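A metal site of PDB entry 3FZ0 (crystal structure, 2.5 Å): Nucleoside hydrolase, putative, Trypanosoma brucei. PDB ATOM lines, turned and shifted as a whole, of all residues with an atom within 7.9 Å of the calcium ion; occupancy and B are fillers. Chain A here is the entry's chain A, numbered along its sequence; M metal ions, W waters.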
ATOM      1  N   ASP A  12      -1.239  14.142   6.522  1.00  0.00           N
ATOM      2  CA  ASP A  12      -0.597  14.741   5.345  1.00  0.00           C
ATOM      3  C   ASP A  12      -0.646  16.253   5.514  1.00  0.00           C
ATOM      4  O   ASP A  12      -1.708  16.831   5.787  1.00  0.00           O
ATOM      5  CB  ASP A  12      -1.263  14.272   4.061  1.00  0.00           C
ATOM      6  CG  ASP A  12      -0.467  14.636   2.833  1.00  0.00           C
ATOM      7  OD1 ASP A  12      -0.767  15.719   2.256  1.00  0.00           O
ATOM      8  OD2 ASP A  12       0.469  13.869   2.459  1.00  0.00           O
ATOM      9  N   THR A  13       0.513  16.895   5.401  1.00  0.00           N
ATOM     10  CA  THR A  13       0.625  18.269   5.893  1.00  0.00           C
ATOM     11  C   THR A  13       1.615  19.137   5.121  1.00  0.00           C
ATOM     12  O   THR A  13       2.653  18.652   4.632  1.00  0.00           O
ATOM     13  CB  THR A  13       1.006  18.241   7.419  1.00  0.00           C
ATOM     14  OG1 THR A  13       1.160  19.570   7.928  1.00  0.00           O
ATOM     15  CG2 THR A  13       2.297  17.475   7.633  1.00  0.00           C
ATOM     16  N   ASP A  14       1.305  20.430   5.016  1.00  0.00           N
ATOM     17  CA  ASP A  14       2.291  21.375   4.513  1.00  0.00           C
ATOM     18  C   ASP A  14       3.033  22.167   5.579  1.00  0.00           C
ATOM     19  O   ASP A  14       3.636  23.183   5.265  1.00  0.00           O
ATOM     20  CB  ASP A  14       1.739  22.280   3.413  1.00  0.00           C
ATOM     21  CG  ASP A  14       0.693  23.233   3.915  1.00  0.00           C
ATOM     22  OD1 ASP A  14       0.072  22.967   4.974  1.00  0.00           O
ATOM     23  OD2 ASP A  14       0.508  24.269   3.241  1.00  0.00           O
ATOM     24  N   CYS A  15       2.933  21.725   6.837  1.00  0.00           N
ATOM     25  CA  CYS A  15       3.878  22.098   7.896  1.00  0.00           C
ATOM     26  C   CYS A  15       3.922  23.559   8.354  1.00  0.00           C
ATOM     27  O   CYS A  15       4.985  24.068   8.739  1.00  0.00           O
ATOM     28  CB  CYS A  15       5.280  21.660   7.515  1.00  0.00           C
ATOM     29  SG  CYS A  15       5.255  19.972   6.853  1.00  0.00           S
ATOM     30  N   GLY A  16       2.764  24.213   8.342  1.00  0.00           N
ATOM     31  CA  GLY A  16       2.669  25.574   8.880  1.00  0.00           C
ATOM     32  C   GLY A  16       2.308  25.564  10.360  1.00  0.00           C
ATOM     33  O   GLY A  16       2.296  24.502  11.032  1.00  0.00           O
ATOM     34  N   GLY A  17       1.951  26.743  10.854  1.00  0.00           N
ATOM     35  CA  GLY A  17       1.683  26.920  12.274  1.00  0.00           C
ATOM     36  C   GLY A  17       0.452  26.203  12.749  1.00  0.00           C
ATOM     37  O   GLY A  17       0.493  25.584  13.823  1.00  0.00           O
ATOM     38  N   ASP A  18      -0.637  26.266  11.980  1.00  0.00           N
ATOM     39  CA  ASP A  18      -1.833  25.515  12.385  1.00  0.00           C
ATOM     40  C   ASP A  18      -1.680  24.026  12.165  1.00  0.00           C
ATOM     41  O   ASP A  18      -2.255  23.237  12.909  1.00  0.00           O
ATOM     42  CB  ASP A  18      -3.151  26.052  11.814  1.00  0.00           C
ATOM     43  CG  ASP A  18      -3.227  25.999  10.293  1.00  0.00           C
ATOM     44  OD1 ASP A  18      -2.238  26.412   9.607  1.00  0.00           O
ATOM     45  OD2 ASP A  18      -4.291  25.566   9.783  1.00  0.00           O
ATOM     46  N   ASP A  19      -0.858  23.638  11.203  1.00  0.00           N
ATOM     47  CA  ASP A  19      -0.501  22.202  11.046  1.00  0.00           C
ATOM     48  C   ASP A  19       0.135  21.678  12.316  1.00  0.00           C
ATOM     49  O   ASP A  19      -0.238  20.602  12.776  1.00  0.00           O
ATOM     50  CB  ASP A  19       0.427  21.946   9.853  1.00  0.00           C
ATOM     51  CG  ASP A  19      -0.157  22.447   8.512  1.00  0.00           C
ATOM     52  OD1 ASP A  19      -0.161  23.676   8.288  1.00  0.00           O
ATOM     53  OD2 ASP A  19      -0.616  21.641   7.684  1.00  0.00           O
ATOM     54  N   ALA A  20       1.055  22.439  12.916  1.00  0.00           N
ATOM     55  CA  ALA A  20       1.698  22.013  14.180  1.00  0.00           C
ATOM     56  C   ALA A  20       0.718  21.856  15.333  1.00  0.00           C
ATOM     57  O   ALA A  20       0.773  20.854  16.039  1.00  0.00           O
ATOM     58  CB  ALA A  20       2.837  22.953  14.583  1.00  0.00           C
ATOM     59  N   ALA A  22      -2.384  21.246  15.071  1.00  0.00           N
ATOM     60  CA  ALA A  22      -3.183  20.078  14.684  1.00  0.00           C
ATOM     61  C   ALA A  22      -2.519  18.754  15.015  1.00  0.00           C
ATOM     62  O   ALA A  22      -3.171  17.848  15.524  1.00  0.00           O
ATOM     63  CB  ALA A  22      -3.532  20.131  13.221  1.00  0.00           C
ATOM     64  N   VAL A  40       3.871  17.710   2.258  1.00  0.00           N
ATOM     65  CA  VAL A  40       3.467  18.192   0.924  1.00  0.00           C
ATOM     66  C   VAL A  40       3.777  19.689   0.836  1.00  0.00           C
ATOM     67  O   VAL A  40       3.783  20.381   1.844  1.00  0.00           O
ATOM     68  CB  VAL A  40       1.946  17.887   0.652  1.00  0.00           C
ATOM     69  CG1 VAL A  40       1.017  18.675   1.562  1.00  0.00           C
ATOM     70  CG2 VAL A  40       1.594  18.108  -0.820  1.00  0.00           C
ATOM     71  N   TRP A  41       4.049  20.159  -0.373  1.00  0.00           N
ATOM     72  CA  TRP A  41       4.267  21.579  -0.631  1.00  0.00           C
ATOM     73  C   TRP A  41       3.006  22.368  -0.242  1.00  0.00           C
ATOM     74  O   TRP A  41       1.951  21.787  -0.084  1.00  0.00           O
ATOM     75  CB  TRP A  41       4.577  21.777  -2.114  1.00  0.00           C
ATOM     76  CG  TRP A  41       3.354  21.606  -2.970  1.00  0.00           C
ATOM     77  CD1 TRP A  41       2.801  20.428  -3.396  1.00  0.00           C
ATOM     78  CD2 TRP A  41       2.489  22.637  -3.459  1.00  0.00           C
ATOM     79  NE1 TRP A  41       1.663  20.657  -4.122  1.00  0.00           N
ATOM     80  CE2 TRP A  41       1.450  22.003  -4.196  1.00  0.00           C
ATOM     81  CE3 TRP A  41       2.503  24.037  -3.368  1.00  0.00           C
ATOM     82  CZ2 TRP A  41       0.436  22.716  -4.841  1.00  0.00           C
ATOM     83  CZ3 TRP A  41       1.474  24.736  -3.991  1.00  0.00           C
ATOM     84  CH2 TRP A  41       0.463  24.077  -4.729  1.00  0.00           C
ATOM     85  N   GLY A  42       3.107  23.671  -0.107  1.00  0.00           N
ATOM     86  CA  GLY A  42       1.974  24.503   0.209  1.00  0.00           C
ATOM     87  C   GLY A  42       2.392  25.865   0.747  1.00  0.00           C
ATOM     88  O   GLY A  42       2.882  26.693  -0.003  1.00  0.00           O
ATOM     89  N   ASN A  43       2.206  26.102   2.037  1.00  0.00           N
ATOM     90  CA  ASN A  43       2.643  27.327   2.596  1.00  0.00           C
ATOM     91  C   ASN A  43       4.160  27.420   2.803  1.00  0.00           C
ATOM     92  O   ASN A  43       4.735  28.512   2.864  1.00  0.00           O
ATOM     93  CB  ASN A  43       1.841  27.664   3.826  1.00  0.00           C
ATOM     94  CG  ASN A  43       0.518  28.334   3.457  1.00  0.00           C
ATOM     95  OD1 ASN A  43       0.474  29.265   2.619  1.00  0.00           O
ATOM     96  ND2 ASN A  43      -0.561  27.842   4.045  1.00  0.00           N
ATOM     97  N   PHE A  86       2.675  32.909   9.165  1.00  0.00           N
ATOM     98  CA  PHE A  86       3.420  32.329  10.275  1.00  0.00           C
ATOM     99  C   PHE A  86       4.911  32.665  10.245  1.00  0.00           C
ATOM    100  O   PHE A  86       5.666  32.199  11.123  1.00  0.00           O
ATOM    101  CB  PHE A  86       3.213  30.804  10.355  1.00  0.00           C
ATOM    102  CG  PHE A  86       1.919  30.418  11.014  1.00  0.00           C
ATOM    103  CD1 PHE A  86       0.811  30.054  10.232  1.00  0.00           C
ATOM    104  CD2 PHE A  86       1.778  30.456  12.401  1.00  0.00           C
ATOM    105  CE1 PHE A  86      -0.418  29.716  10.833  1.00  0.00           C
ATOM    106  CE2 PHE A  86       0.570  30.124  13.011  1.00  0.00           C
ATOM    107  CZ  PHE A  86      -0.530  29.747  12.217  1.00  0.00           C
ATOM    108  N   ALA A 133      -5.925  15.127   5.965  1.00  0.00           N
ATOM    109  CA  ALA A 133      -5.124  15.919   5.014  1.00  0.00           C
ATOM    110  C   ALA A 133      -5.198  17.433   5.353  1.00  0.00           C
ATOM    111  O   ALA A 133      -6.278  18.040   5.405  1.00  0.00           O
ATOM    112  CB  ALA A 133      -5.569  15.644   3.588  1.00  0.00           C
ATOM    113  N   LEU A 134      -4.029  18.019   5.607  1.00  0.00           N
ATOM    114  CA  LEU A 134      -3.954  19.413   6.099  1.00  0.00           C
ATOM    115  C   LEU A 134      -3.291  20.345   5.100  1.00  0.00           C
ATOM    116  O   LEU A 134      -2.905  21.466   5.446  1.00  0.00           O
ATOM    117  CB  LEU A 134      -3.223  19.473   7.447  1.00  0.00           C
ATOM    118  CG  LEU A 134      -3.743  18.506   8.530  1.00  0.00           C
ATOM    119  CD1 LEU A 134      -2.882  18.623   9.774  1.00  0.00           C
ATOM    120  CD2 LEU A 134      -5.265  18.726   8.815  1.00  0.00           C
ATOM    121  N   GLY A 135      -3.152  19.906   3.856  1.00  0.00           N
ATOM    122  CA  GLY A 135      -2.493  20.752   2.868  1.00  0.00           C
ATOM    123  C   GLY A 135      -3.098  20.482   1.520  1.00  0.00           C
ATOM    124  O   GLY A 135      -4.145  19.853   1.463  1.00  0.00           O
ATOM    125  N   PRO A 136      -2.446  20.955   0.448  1.00  0.00           N
ATOM    126  CA  PRO A 136      -2.826  20.543  -0.887  1.00  0.00           C
ATOM    127  C   PRO A 136      -2.883  19.009  -0.992  1.00  0.00           C
ATOM    128  O   PRO A 136      -2.041  18.341  -0.413  1.00  0.00           O
ATOM    129  CB  PRO A 136      -1.684  21.071  -1.747  1.00  0.00           C
ATOM    130  CG  PRO A 136      -1.172  22.253  -1.009  1.00  0.00           C
ATOM    131  CD  PRO A 136      -1.306  21.879   0.437  1.00  0.00           C
ATOM    132  N   MET A 165      -8.815  19.262   5.500  1.00  0.00           N
ATOM    133  CA  MET A 165      -9.013  20.694   5.630  1.00  0.00           C
ATOM    134  C   MET A 165      -8.860  21.276   4.214  1.00  0.00           C
ATOM    135  O   MET A 165      -7.772  21.334   3.660  1.00  0.00           O
ATOM    136  CB  MET A 165      -8.025  21.331   6.620  1.00  0.00           C
ATOM    137  CG  MET A 165      -8.447  22.735   7.076  1.00  0.00           C
ATOM    138  SD  MET A 165      -8.253  23.964   5.760  1.00  0.00           S
ATOM    139  CE  MET A 165      -9.846  24.805   5.793  1.00  0.00           C
ATOM    140  N   GLU A 180     -10.550  28.366  -1.473  1.00  0.00           N
ATOM    141  CA  GLU A 180      -9.696  28.258  -0.297  1.00  0.00           C
ATOM    142  C   GLU A 180      -8.302  27.796  -0.727  1.00  0.00           C
ATOM    143  O   GLU A 180      -8.162  27.098  -1.734  1.00  0.00           O
ATOM    144  CB  GLU A 180     -10.338  27.277   0.689  1.00  0.00           C
ATOM    145  CG  GLU A 180      -9.549  27.012   1.981  1.00  0.00           C
ATOM    146  CD  GLU A 180      -8.432  25.966   1.800  1.00  0.00           C
ATOM    147  OE1 GLU A 180      -8.599  25.025   1.013  1.00  0.00           O
ATOM    148  OE2 GLU A 180      -7.367  26.107   2.430  1.00  0.00           O
ATOM    149  N   PHE A 181      -7.275  28.193   0.021  1.00  0.00           N
ATOM    150  CA  PHE A 181      -5.858  27.913  -0.309  1.00  0.00           C
ATOM    151  C   PHE A 181      -5.536  26.479  -0.757  1.00  0.00           C
ATOM    152  O   PHE A 181      -5.021  26.250  -1.887  1.00  0.00           O
ATOM    153  CB  PHE A 181      -4.921  28.334   0.842  1.00  0.00           C
ATOM    154  CG  PHE A 181      -3.456  28.146   0.561  1.00  0.00           C
ATOM    155  CD1 PHE A 181      -2.740  29.067  -0.245  1.00  0.00           C
ATOM    156  CD2 PHE A 181      -2.774  27.082   1.137  1.00  0.00           C
ATOM    157  CE1 PHE A 181      -1.352  28.904  -0.495  1.00  0.00           C
ATOM    158  CE2 PHE A 181      -1.389  26.906   0.917  1.00  0.00           C
ATOM    159  CZ  PHE A 181      -0.674  27.811   0.078  1.00  0.00           C
ATOM    160  N   ASN A 182      -5.823  25.522   0.132  1.00  0.00           N
ATOM    161  CA  ASN A 182      -5.464  24.120  -0.116  1.00  0.00           C
ATOM    162  C   ASN A 182      -6.114  23.645  -1.397  1.00  0.00           C
ATOM    163  O   ASN A 182      -5.479  22.977  -2.209  1.00  0.00           O
ATOM    164  CB  ASN A 182      -5.840  23.188   1.055  1.00  0.00           C
ATOM    165  CG  ASN A 182      -4.950  23.390   2.291  1.00  0.00           C
ATOM    166  OD1 ASN A 182      -3.831  23.927   2.217  1.00  0.00           O
ATOM    167  ND2 ASN A 182      -5.429  22.925   3.436  1.00  0.00           N
ATOM    168  N   PRO A 282      -7.401  26.536  11.392  1.00  0.00           N
ATOM    169  CA  PRO A 282      -8.163  25.571  10.586  1.00  0.00           C
ATOM    170  C   PRO A 282      -7.751  24.087  10.649  1.00  0.00           C
ATOM    171  O   PRO A 282      -8.619  23.221  10.786  1.00  0.00           O
ATOM    172  CB  PRO A 282      -7.998  26.117   9.169  1.00  0.00           C
ATOM    173  CG  PRO A 282      -7.869  27.559   9.387  1.00  0.00           C
ATOM    174  CD  PRO A 282      -6.930  27.649  10.550  1.00  0.00           C
ATOM    175  N   ASP A 283      -6.452  23.785  10.546  1.00  0.00           N
ATOM    176  CA  ASP A 283      -6.047  22.384  10.576  1.00  0.00           C
ATOM    177  C   ASP A 283      -6.416  21.677  11.902  1.00  0.00           C
ATOM    178  O   ASP A 283      -6.739  20.492  11.923  1.00  0.00           O
ATOM    179  CB  ASP A 283      -4.569  22.229  10.284  1.00  0.00           C
ATOM    180  CG  ASP A 283      -4.198  22.624   8.858  1.00  0.00           C
ATOM    181  OD1 ASP A 283      -5.091  22.571   7.982  1.00  0.00           O
ATOM    182  OD2 ASP A 283      -3.022  22.966   8.610  1.00  0.00           O
HETATM  183 CA    CA M   1      -1.963  23.431   6.410  1.00  0.00          CA
HETATM  184  O   HOH W   1      -1.681  25.621   7.197  1.00  0.00           O
HETATM  185  O   HOH W   2      -1.860  24.769   4.287  1.00  0.00           O
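Water W2 lies within hydrogen-bond range of OD2 of Asp 14 (2.6 Å), OD1 of Asn 182 (3.0 Å) and ND2 of Asn 43 (3.3 Å).
OG1 of Thr 13 lies close to OD2 of Asp 19, at 2.7 Å.
The side-chain carboxylate of Asp 18 sits at hydrogen-bond distance from the backbone NH of Asp 283 (2.9 Å).
The side-chain carboxylate (OD2) of Asp 14 lies within hydrogen-bond range of the backbone NH (N) of Asn 43 (2.8 Å).
O of Asp 12 lies within hydrogen-bond range of N of Leu 134.
The side-chain carboxylate of Asp 19 lies close to the backbone NH of Gly 16, 3.0 Å away.
Four residues have an atom within 4 Å of the calcium ion: Asp 14, Asp 19, Leu 134 and Asp 283.
The calcium ion is bound by water W1, the backbone carbonyl oxygen (O) of Leu 134, the side-chain carboxylate (OD2) of Asp 283, water W2, the side-chain carboxylate (OD1) of Asp 14, the side-chain carboxylate (OD2) of Asp 19 and the side-chain carboxylate (OD1) of Asp 19.
The calcium ion has seven donor atoms within binding distance.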
